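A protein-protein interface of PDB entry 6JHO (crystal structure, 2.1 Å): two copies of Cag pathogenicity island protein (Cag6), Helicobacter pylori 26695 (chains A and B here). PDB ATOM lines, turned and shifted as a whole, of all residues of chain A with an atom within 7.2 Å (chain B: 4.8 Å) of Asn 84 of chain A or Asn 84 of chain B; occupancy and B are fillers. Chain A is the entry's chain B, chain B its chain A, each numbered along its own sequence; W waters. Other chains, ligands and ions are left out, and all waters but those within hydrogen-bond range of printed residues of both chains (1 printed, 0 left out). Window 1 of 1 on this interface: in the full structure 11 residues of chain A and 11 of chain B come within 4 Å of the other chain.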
ATOM      1  N   ILE A  22       9.414  -3.083  28.341  1.00  0.00           N
ATOM      2  CA  ILE A  22       9.085  -1.660  28.394  1.00  0.00           C
ATOM      3  C   ILE A  22       9.692  -0.931  27.204  1.00  0.00           C
ATOM      4  O   ILE A  22       9.038  -0.097  26.568  1.00  0.00           O
ATOM      5  CB  ILE A  22       9.544  -1.068  29.738  1.00  0.00           C
ATOM      6  CG1 ILE A  22       8.670  -1.613  30.875  1.00  0.00           C
ATOM      7  CG2 ILE A  22       9.495   0.443  29.712  1.00  0.00           C
ATOM      8  CD1 ILE A  22       9.153  -1.260  32.277  1.00  0.00           C
ATOM      9  N   SER A  25       7.558  -1.972  24.196  1.00  0.00           N
ATOM     10  CA  SER A  25       6.233  -1.367  24.193  1.00  0.00           C
ATOM     11  C   SER A  25       6.258   0.132  23.896  1.00  0.00           C
ATOM     12  O   SER A  25       5.200   0.712  23.640  1.00  0.00           O
ATOM     13  CB  SER A  25       5.557  -1.648  25.536  1.00  0.00           C
ATOM     14  OG  SER A  25       4.698  -0.593  25.903  1.00  0.00           O
ATOM     15  N   ASN A  26       7.429   0.766  23.889  1.00  0.00           N
ATOM     16  CA  ASN A  26       7.518   2.204  23.698  1.00  0.00           C
ATOM     17  C   ASN A  26       8.392   2.591  22.521  1.00  0.00           C
ATOM     18  O   ASN A  26       8.509   3.783  22.223  1.00  0.00           O
ATOM     19  CB  ASN A  26       8.038   2.874  24.978  1.00  0.00           C
ATOM     20  CG  ASN A  26       6.958   3.040  26.012  1.00  0.00           C
ATOM     21  OD1 ASN A  26       6.113   3.921  25.884  1.00  0.00           O
ATOM     22  ND2 ASN A  26       6.946   2.171  27.031  1.00  0.00           N
ATOM     23  N   LEU A  29       7.533   5.196  19.140  1.00  0.00           N
ATOM     24  CA  LEU A  29       7.850   6.620  19.059  1.00  0.00           C
ATOM     25  C   LEU A  29       9.290   6.850  18.606  1.00  0.00           C
ATOM     26  O   LEU A  29       9.563   7.751  17.802  1.00  0.00           O
ATOM     27  CB  LEU A  29       7.603   7.279  20.417  1.00  0.00           C
ATOM     28  CG  LEU A  29       6.181   7.229  20.974  1.00  0.00           C
ATOM     29  CD1 LEU A  29       5.159   7.389  19.855  1.00  0.00           C
ATOM     30  CD2 LEU A  29       5.925   5.963  21.797  1.00  0.00           C
ATOM     31  N   VAL A  77       8.470  14.441  21.119  1.00  0.00           N
ATOM     32  CA  VAL A  77       8.305  12.990  21.059  1.00  0.00           C
ATOM     33  C   VAL A  77       9.315  12.303  21.970  1.00  0.00           C
ATOM     34  O   VAL A  77       9.009  11.288  22.613  1.00  0.00           O
ATOM     35  CB  VAL A  77       8.434  12.499  19.607  1.00  0.00           C
ATOM     36  CG1 VAL A  77       8.383  10.998  19.552  1.00  0.00           C
ATOM     37  CG2 VAL A  77       7.325  13.120  18.742  1.00  0.00           C
ATOM     38  N   TYR A  78      10.530  12.842  22.037  1.00  0.00           N
ATOM     39  CA  TYR A  78      11.560  12.204  22.853  1.00  0.00           C
ATOM     40  C   TYR A  78      11.285  12.423  24.326  1.00  0.00           C
ATOM     41  O   TYR A  78      11.555  11.546  25.153  1.00  0.00           O
ATOM     42  CB  TYR A  78      12.944  12.737  22.473  1.00  0.00           C
ATOM     43  CG  TYR A  78      13.260  12.532  21.011  1.00  0.00           C
ATOM     44  CD1 TYR A  78      12.733  11.453  20.326  1.00  0.00           C
ATOM     45  CD2 TYR A  78      14.062  13.412  20.314  1.00  0.00           C
ATOM     46  CE1 TYR A  78      12.998  11.241  18.983  1.00  0.00           C
ATOM     47  CE2 TYR A  78      14.342  13.211  18.963  1.00  0.00           C
ATOM     48  CZ  TYR A  78      13.800  12.121  18.297  1.00  0.00           C
ATOM     49  OH  TYR A  78      14.054  11.898  16.948  1.00  0.00           O
ATOM     50  N   TYR A  79      10.744  13.591  24.672  1.00  0.00           N
ATOM     51  CA  TYR A  79      10.399  13.860  26.061  1.00  0.00           C
ATOM     52  C   TYR A  79       9.242  12.969  26.517  1.00  0.00           C
ATOM     53  O   TYR A  79       9.280  12.414  27.622  1.00  0.00           O
ATOM     54  CB  TYR A  79      10.090  15.350  26.208  1.00  0.00           C
ATOM     55  CG  TYR A  79       9.395  15.742  27.485  1.00  0.00           C
ATOM     56  CD1 TYR A  79      10.109  16.106  28.623  1.00  0.00           C
ATOM     57  CD2 TYR A  79       8.009  15.759  27.547  1.00  0.00           C
ATOM     58  CE1 TYR A  79       9.452  16.462  29.796  1.00  0.00           C
ATOM     59  CE2 TYR A  79       7.355  16.112  28.697  1.00  0.00           C
ATOM     60  CZ  TYR A  79       8.070  16.462  29.815  1.00  0.00           C
ATOM     61  OH  TYR A  79       7.341  16.814  30.935  1.00  0.00           O
ATOM     62  N   ASN A  80       8.223  12.798  25.665  1.00  0.00           N
ATOM     63  CA  ASN A  80       7.112  11.882  25.950  1.00  0.00           C
ATOM     64  C   ASN A  80       7.598  10.466  26.157  1.00  0.00           C
ATOM     65  O   ASN A  80       7.084   9.744  27.018  1.00  0.00           O
ATOM     66  CB  ASN A  80       6.115  11.851  24.791  1.00  0.00           C
ATOM     67  CG  ASN A  80       5.199  12.990  24.809  1.00  0.00           C
ATOM     68  OD1 ASN A  80       5.293  13.844  25.689  1.00  0.00           O
ATOM     69  ND2 ASN A  80       4.299  13.050  23.822  1.00  0.00           N
ATOM     70  N   TYR A  81       8.533  10.030  25.315  1.00  0.00           N
ATOM     71  CA  TYR A  81       9.061   8.679  25.414  1.00  0.00           C
ATOM     72  C   TYR A  81       9.690   8.445  26.782  1.00  0.00           C
ATOM     73  O   TYR A  81       9.440   7.421  27.428  1.00  0.00           O
ATOM     74  CB  TYR A  81      10.077   8.459  24.301  1.00  0.00           C
ATOM     75  CG  TYR A  81      10.956   7.241  24.451  1.00  0.00           C
ATOM     76  CD1 TYR A  81      10.490   5.967  24.128  1.00  0.00           C
ATOM     77  CD2 TYR A  81      12.267   7.366  24.909  1.00  0.00           C
ATOM     78  CE1 TYR A  81      11.316   4.848  24.249  1.00  0.00           C
ATOM     79  CE2 TYR A  81      13.094   6.263  25.028  1.00  0.00           C
ATOM     80  CZ  TYR A  81      12.617   5.009  24.700  1.00  0.00           C
ATOM     81  OH  TYR A  81      13.448   3.922  24.827  1.00  0.00           O
ATOM     82  N   LEU A  82      10.492   9.408  27.245  1.00  0.00           N
ATOM     83  CA  LEU A  82      11.143   9.278  28.543  1.00  0.00           C
ATOM     84  C   LEU A  82      10.115   9.257  29.669  1.00  0.00           C
ATOM     85  O   LEU A  82      10.244   8.476  30.619  1.00  0.00           O
ATOM     86  CB  LEU A  82      12.162  10.412  28.744  1.00  0.00           C
ATOM     87  CG  LEU A  82      13.463  10.341  27.935  1.00  0.00           C
ATOM     88  CD1 LEU A  82      14.344  11.598  28.128  1.00  0.00           C
ATOM     89  CD2 LEU A  82      14.251   9.077  28.284  1.00  0.00           C
ATOM     90  N   ASN A  83       9.066  10.084  29.567  1.00  0.00           N
ATOM     91  CA  ASN A  83       7.999  10.051  30.568  1.00  0.00           C
ATOM     92  C   ASN A  83       7.287   8.703  30.580  1.00  0.00           C
ATOM     93  O   ASN A  83       6.924   8.200  31.651  1.00  0.00           O
ATOM     94  CB  ASN A  83       6.982  11.161  30.316  1.00  0.00           C
ATOM     95  CG  ASN A  83       7.362  12.471  30.974  1.00  0.00           C
ATOM     96  OD1 ASN A  83       8.107  12.492  31.949  1.00  0.00           O
ATOM     97  ND2 ASN A  83       6.831  13.571  30.452  1.00  0.00           N
ATOM     98  N   ASN A  84       7.026   8.139  29.389  1.00  0.00           N
ATOM     99  CA  ASN A  84       6.439   6.806  29.286  1.00  0.00           C
ATOM    100  C   ASN A  84       7.326   5.778  29.981  1.00  0.00           C
ATOM    101  O   ASN A  84       6.831   4.898  30.696  1.00  0.00           O
ATOM    102  CB  ASN A  84       6.255   6.391  27.809  1.00  0.00           C
ATOM    103  CG  ASN A  84       5.274   7.295  27.018  1.00  0.00           C
ATOM    104  OD1 ASN A  84       4.483   8.035  27.579  1.00  0.00           O
ATOM    105  ND2 ASN A  84       5.327   7.188  25.689  1.00  0.00           N
ATOM    106  N   LEU A  85       8.644   5.842  29.725  1.00  0.00           N
ATOM    107  CA  LEU A  85       9.579   4.900  30.324  1.00  0.00           C
ATOM    108  C   LEU A  85       9.586   5.005  31.841  1.00  0.00           C
ATOM    109  O   LEU A  85       9.553   3.980  32.530  1.00  0.00           O
ATOM    110  CB  LEU A  85      10.993   5.123  29.803  1.00  0.00           C
ATOM    111  CG  LEU A  85      11.330   4.690  28.386  1.00  0.00           C
ATOM    112  CD1 LEU A  85      12.851   4.691  28.185  1.00  0.00           C
ATOM    113  CD2 LEU A  85      10.717   3.345  28.098  1.00  0.00           C
ATOM    114  N   VAL A  86       9.693   6.230  32.376  1.00  0.00           N
ATOM    115  CA  VAL A  86       9.797   6.398  33.823  1.00  0.00           C
ATOM    116  C   VAL A  86       8.584   5.797  34.505  1.00  0.00           C
ATOM    117  O   VAL A  86       8.704   5.112  35.524  1.00  0.00           O
ATOM    118  CB  VAL A  86       9.944   7.882  34.213  1.00  0.00           C
ATOM    119  CG1 VAL A  86       9.986   8.010  35.733  1.00  0.00           C
ATOM    120  CG2 VAL A  86      11.203   8.466  33.655  1.00  0.00           C
ATOM    121  N   LEU A  87       7.397   6.043  33.945  1.00  0.00           N
ATOM    122  CA  LEU A  87       6.168   5.611  34.595  1.00  0.00           C
ATOM    123  C   LEU A  87       6.007   4.098  34.533  1.00  0.00           C
ATOM    124  O   LEU A  87       5.606   3.467  35.526  1.00  0.00           O
ATOM    125  CB  LEU A  87       4.967   6.301  33.948  1.00  0.00           C
ATOM    126  CG  LEU A  87       3.762   6.329  34.881  1.00  0.00           C
ATOM    127  CD1 LEU A  87       3.830   7.579  35.750  1.00  0.00           C
ATOM    128  CD2 LEU A  87       2.489   6.300  34.083  1.00  0.00           C
ATOM    129  N   ALA A  88       6.303   3.495  33.379  1.00  0.00           N
ATOM    130  CA  ALA A  88       6.218   2.037  33.260  1.00  0.00           C
ATOM    131  C   ALA A  88       7.258   1.344  34.141  1.00  0.00           C
ATOM    132  O   ALA A  88       6.940   0.360  34.827  1.00  0.00           O
ATOM    133  CB  ALA A  88       6.381   1.623  31.788  1.00  0.00           C
ATOM    134  N   SER A  89       8.503   1.853  34.132  1.00  0.00           N
ATOM    135  CA  SER A  89       9.586   1.315  34.967  1.00  0.00           C
ATOM    136  C   SER A  89       9.257   1.425  36.448  1.00  0.00           C
ATOM    137  O   SER A  89       9.446   0.474  37.216  1.00  0.00           O
ATOM    138  CB  SER A  89      10.898   2.064  34.690  1.00  0.00           C
ATOM    139  OG  SER A  89      11.299   1.905  33.345  1.00  0.00           O
ATOM    140  N   TYR A  90       8.833   2.610  36.882  1.00  0.00           N
ATOM    141  CA  TYR A  90       8.523   2.786  38.287  1.00  0.00           C
ATOM    142  C   TYR A  90       7.379   1.873  38.705  1.00  0.00           C
ATOM    143  O   TYR A  90       7.427   1.261  39.783  1.00  0.00           O
ATOM    144  CB  TYR A  90       8.198   4.251  38.579  1.00  0.00           C
ATOM    145  CG  TYR A  90       7.827   4.465  40.018  1.00  0.00           C
ATOM    146  CD1 TYR A  90       8.804   4.431  41.013  1.00  0.00           C
ATOM    147  CD2 TYR A  90       6.496   4.669  40.398  1.00  0.00           C
ATOM    148  CE1 TYR A  90       8.476   4.599  42.355  1.00  0.00           C
ATOM    149  CE2 TYR A  90       6.149   4.852  41.740  1.00  0.00           C
ATOM    150  CZ  TYR A  90       7.147   4.810  42.712  1.00  0.00           C
ATOM    151  OH  TYR A  90       6.823   4.987  44.045  1.00  0.00           O
ATOM    152  N   MET A 125      16.818   3.902  33.621  1.00  0.00           N
ATOM    153  CA  MET A 125      16.324   5.243  33.317  1.00  0.00           C
ATOM    154  C   MET A 125      17.466   6.192  32.955  1.00  0.00           C
ATOM    155  O   MET A 125      17.382   6.935  31.971  1.00  0.00           O
ATOM    156  CB  MET A 125      15.525   5.794  34.506  1.00  0.00           C
ATOM    157  CG  MET A 125      14.088   5.285  34.590  1.00  0.00           C
ATOM    158  SD  MET A 125      13.201   5.188  33.009  1.00  0.00           S
ATOM    159  CE  MET A 125      13.585   6.756  32.199  1.00  0.00           C
ATOM    160  N   ASN B  26      -2.593   3.332  22.414  1.00  0.00           N
ATOM    161  CA  ASN B  26      -2.411   3.793  23.785  1.00  0.00           C
ATOM    162  C   ASN B  26      -3.427   3.172  24.735  1.00  0.00           C
ATOM    163  O   ASN B  26      -3.560   3.627  25.872  1.00  0.00           O
ATOM    164  CB  ASN B  26      -2.486   5.318  23.838  1.00  0.00           C
ATOM    165  CG  ASN B  26      -1.365   5.972  23.072  1.00  0.00           C
ATOM    166  OD1 ASN B  26      -0.254   6.092  23.585  1.00  0.00           O
ATOM    167  ND2 ASN B  26      -1.643   6.410  21.846  1.00  0.00           N
ATOM    168  N   LEU B  29      -2.351   1.718  28.457  1.00  0.00           N
ATOM    169  CA  LEU B  29      -2.136   2.621  29.583  1.00  0.00           C
ATOM    170  C   LEU B  29      -3.401   2.780  30.421  1.00  0.00           C
ATOM    171  O   LEU B  29      -3.343   2.780  31.655  1.00  0.00           O
ATOM    172  CB  LEU B  29      -1.654   3.985  29.071  1.00  0.00           C
ATOM    173  CG  LEU B  29      -0.359   4.142  28.256  1.00  0.00           C
ATOM    174  CD1 LEU B  29      -0.376   3.404  26.920  1.00  0.00           C
ATOM    175  CD2 LEU B  29      -0.077   5.620  28.016  1.00  0.00           C
ATOM    176  N   ASN B  80       0.059  11.373  30.910  1.00  0.00           N
ATOM    177  CA  ASN B  80       0.894  10.841  29.830  1.00  0.00           C
ATOM    178  C   ASN B  80       0.051  10.373  28.669  1.00  0.00           C
ATOM    179  O   ASN B  80       0.392  10.614  27.510  1.00  0.00           O
ATOM    180  CB  ASN B  80       1.744   9.656  30.291  1.00  0.00           C
ATOM    181  CG  ASN B  80       2.817  10.056  31.234  1.00  0.00           C
ATOM    182  OD1 ASN B  80       3.114  11.247  31.369  1.00  0.00           O
ATOM    183  ND2 ASN B  80       3.405   9.070  31.934  1.00  0.00           N
ATOM    184  N   TYR B  81      -1.032   9.658  28.970  1.00  0.00           N
ATOM    185  CA  TYR B  81      -1.913   9.167  27.929  1.00  0.00           C
ATOM    186  C   TYR B  81      -2.396  10.310  27.047  1.00  0.00           C
ATOM    187  O   TYR B  81      -2.379  10.198  25.818  1.00  0.00           O
ATOM    188  CB  TYR B  81      -3.089   8.431  28.559  1.00  0.00           C
ATOM    189  CG  TYR B  81      -4.218   8.112  27.605  1.00  0.00           C
ATOM    190  CD1 TYR B  81      -4.133   7.028  26.740  1.00  0.00           C
ATOM    191  CD2 TYR B  81      -5.380   8.872  27.589  1.00  0.00           C
ATOM    192  CE1 TYR B  81      -5.166   6.716  25.882  1.00  0.00           C
ATOM    193  CE2 TYR B  81      -6.417   8.568  26.733  1.00  0.00           C
ATOM    194  CZ  TYR B  81      -6.308   7.488  25.885  1.00  0.00           C
ATOM    195  OH  TYR B  81      -7.343   7.175  25.033  1.00  0.00           O
ATOM    196  N   LEU B  82      -2.795  11.431  27.660  1.00  0.00           N
ATOM    197  CA  LEU B  82      -3.274  12.563  26.871  1.00  0.00           C
ATOM    198  C   LEU B  82      -2.140  13.173  26.051  1.00  0.00           C
ATOM    199  O   LEU B  82      -2.335  13.515  24.876  1.00  0.00           O
ATOM    200  CB  LEU B  82      -3.918  13.610  27.783  1.00  0.00           C
ATOM    201  CG  LEU B  82      -5.272  13.205  28.391  1.00  0.00           C
ATOM    202  CD1 LEU B  82      -5.759  14.232  29.406  1.00  0.00           C
ATOM    203  CD2 LEU B  82      -6.330  12.965  27.284  1.00  0.00           C
ATOM    204  N   ASN B  83      -0.949  13.300  26.644  1.00  0.00           N
ATOM    205  CA  ASN B  83       0.212  13.765  25.890  1.00  0.00           C
ATOM    206  C   ASN B  83       0.502  12.853  24.709  1.00  0.00           C
ATOM    207  O   ASN B  83       0.730  13.326  23.587  1.00  0.00           O
ATOM    208  CB  ASN B  83       1.433  13.864  26.801  1.00  0.00           C
ATOM    209  CG  ASN B  83       1.510  15.198  27.501  1.00  0.00           C
ATOM    210  OD1 ASN B  83       1.034  16.202  26.974  1.00  0.00           O
ATOM    211  ND2 ASN B  83       2.105  15.223  28.686  1.00  0.00           N
ATOM    212  N   ASN B  84       0.490  11.536  24.943  1.00  0.00           N
ATOM    213  CA  ASN B  84       0.655  10.586  23.848  1.00  0.00           C
ATOM    214  C   ASN B  84      -0.360  10.841  22.736  1.00  0.00           C
ATOM    215  O   ASN B  84      -0.005  10.807  21.551  1.00  0.00           O
ATOM    216  CB  ASN B  84       0.507   9.141  24.351  1.00  0.00           C
ATOM    217  CG  ASN B  84       1.601   8.724  25.305  1.00  0.00           C
ATOM    218  OD1 ASN B  84       2.632   9.363  25.412  1.00  0.00           O
ATOM    219  ND2 ASN B  84       1.367   7.613  26.006  1.00  0.00           N
ATOM    220  N   LEU B  85      -1.634  11.091  23.103  1.00  0.00           N
ATOM    221  CA  LEU B  85      -2.684  11.266  22.101  1.00  0.00           C
ATOM    222  C   LEU B  85      -2.476  12.533  21.290  1.00  0.00           C
ATOM    223  O   LEU B  85      -2.619  12.510  20.060  1.00  0.00           O
ATOM    224  CB  LEU B  85      -4.072  11.313  22.740  1.00  0.00           C
ATOM    225  CG  LEU B  85      -4.739  10.052  23.297  1.00  0.00           C
ATOM    226  CD1 LEU B  85      -6.192  10.355  23.625  1.00  0.00           C
ATOM    227  CD2 LEU B  85      -4.663   8.897  22.343  1.00  0.00           C
ATOM    228  N   VAL B  86      -2.166  13.656  21.958  1.00  0.00           N
ATOM    229  CA  VAL B  86      -2.021  14.910  21.219  1.00  0.00           C
ATOM    230  C   VAL B  86      -0.905  14.788  20.201  1.00  0.00           C
ATOM    231  O   VAL B  86      -1.047  15.213  19.053  1.00  0.00           O
ATOM    232  CB  VAL B  86      -1.769  16.108  22.149  1.00  0.00           C
ATOM    233  CG1 VAL B  86      -1.992  17.393  21.366  1.00  0.00           C
ATOM    234  CG2 VAL B  86      -2.694  16.103  23.304  1.00  0.00           C
ATOM    235  N   LEU B  87       0.210  14.181  20.602  1.00  0.00           N
ATOM    236  CA  LEU B  87       1.370  14.090  19.730  1.00  0.00           C
ATOM    237  C   LEU B  87       1.080  13.220  18.521  1.00  0.00           C
ATOM    238  O   LEU B  87       1.358  13.617  17.383  1.00  0.00           O
ATOM    239  CB  LEU B  87       2.570  13.550  20.513  1.00  0.00           C
ATOM    240  CG  LEU B  87       3.292  14.773  21.092  1.00  0.00           C
ATOM    241  CD1 LEU B  87       2.765  15.133  22.502  1.00  0.00           C
ATOM    242  CD2 LEU B  87       4.806  14.612  21.072  1.00  0.00           C
ATOM    243  N   ALA B  88       0.488  12.038  18.744  1.00  0.00           N
ATOM    244  CA  ALA B  88       0.176  11.154  17.624  1.00  0.00           C
ATOM    245  C   ALA B  88      -0.905  11.758  16.737  1.00  0.00           C
ATOM    246  O   ALA B  88      -0.826  11.667  15.504  1.00  0.00           O
ATOM    247  CB  ALA B  88      -0.253   9.776  18.138  1.00  0.00           C
HETATM  248  O   HOH W   1       5.700  10.247  33.885  1.00  0.00           O
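OD1 of Asn 84 of chain A lies close to OD1 of Asn 84 of chain B, 3.1 Å away.
The side-chain amide oxygen of Asn 26 of chain A lies close to the side-chain amide nitrogen of Asn 84 of chain A, 3.4 Å away.
The backbone carbonyl oxygen (O) of Asn 80 of chain A sits close to the side-chain amide oxygen (OD1) of Asn 84 of chain A (3.2 Å).
O of Asn 80 of chain B lies close to OD1 of Asn 84 of chain B (3.3 Å).
The side-chain amide oxygen of Asn 26 of chain B sits close to the side-chain amide nitrogen of Asn 84 of chain B (3.3 Å).
OH of Tyr 79 of chain A lies close to ND2 of Asn 83 of chain A (3.3 Å).
Among the printed residues, merely in contact across the chains: Asn 80 of chain A with Leu 87 of chain B, Asn 80 of chain A with Asn 83 of chain B, Leu 87 of chain A with Asn 80 of chain B, Asn 83 of chain A with Asn 80 of chain B and Val 77 of chain A with Leu 87 of chain B.
Printed residues of chain B within 4 Å of Val 77 of chain A: Leu 87 (3.7 Å).
Of the printed residues of chain B, Asn 83 of chain A touches Asn 80.
Asn 84 of chain A touches just one residue of chain B: Asn 84 (3.1 Å).
Val 86 of chain A touches none of the printed residues of chain B.
Of the printed residues of chain B, Leu 87 of chain A touches Asn 80 (3.6 Å).
Printed residues of chain A within 4 Å of Asn 80 of chain B: Asn 83 and Leu 87.
Tyr 81 of chain B touches none of the printed residues of chain A.
Printed residues of chain A within 4 Å of Asn 83 of chain B: Asn 80 (3.6 Å).
Asn 84 of chain B touches just one residue of chain A: Asn 84 (3.1 Å).
The nearest residue of chain B that does not touch Asn 84 of chain A is Asn 80 of chain B (4.2 Å).
The nearest residue of chain A that does not touch Asn 84 of chain B is Asn 80 of chain A (4.2 Å).
Of the 11 printed residues of chain B, 4 touch a printed residue of chain A.
Of the 19 printed residues of chain A, 5 touch a printed residue of chain B.
Hydrophobic or aromatic side chains of chain A within 4 Å of the printed part of chain B: Val 77 and Leu 87.
Along chain A the printed residues that touch a printed residue of chain B span positions 77 to 87.
Among the printed residues, no Asp or Glu carboxylate lies within 4 Å of a Lys or Arg side-chain nitrogen of the other chain.
Asn 80 of chain A touches Asn 83 of chain B, and with the chains exchanged Asn 83 of chain A touches Asn 80 of chain B.
Asn 80 of chain A touches Leu 87 of chain B, and with the chains exchanged Leu 87 of chain A touches Asn 80 of chain B.
Asn 84 of chain B touches its own counterpart, Asn 84 of chain A.
Water W1 lies within hydrogen-bond range of ND2 of Asn 80 of chain B (3.2 Å) and O of Asn 83 of chain A (3.3 Å).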
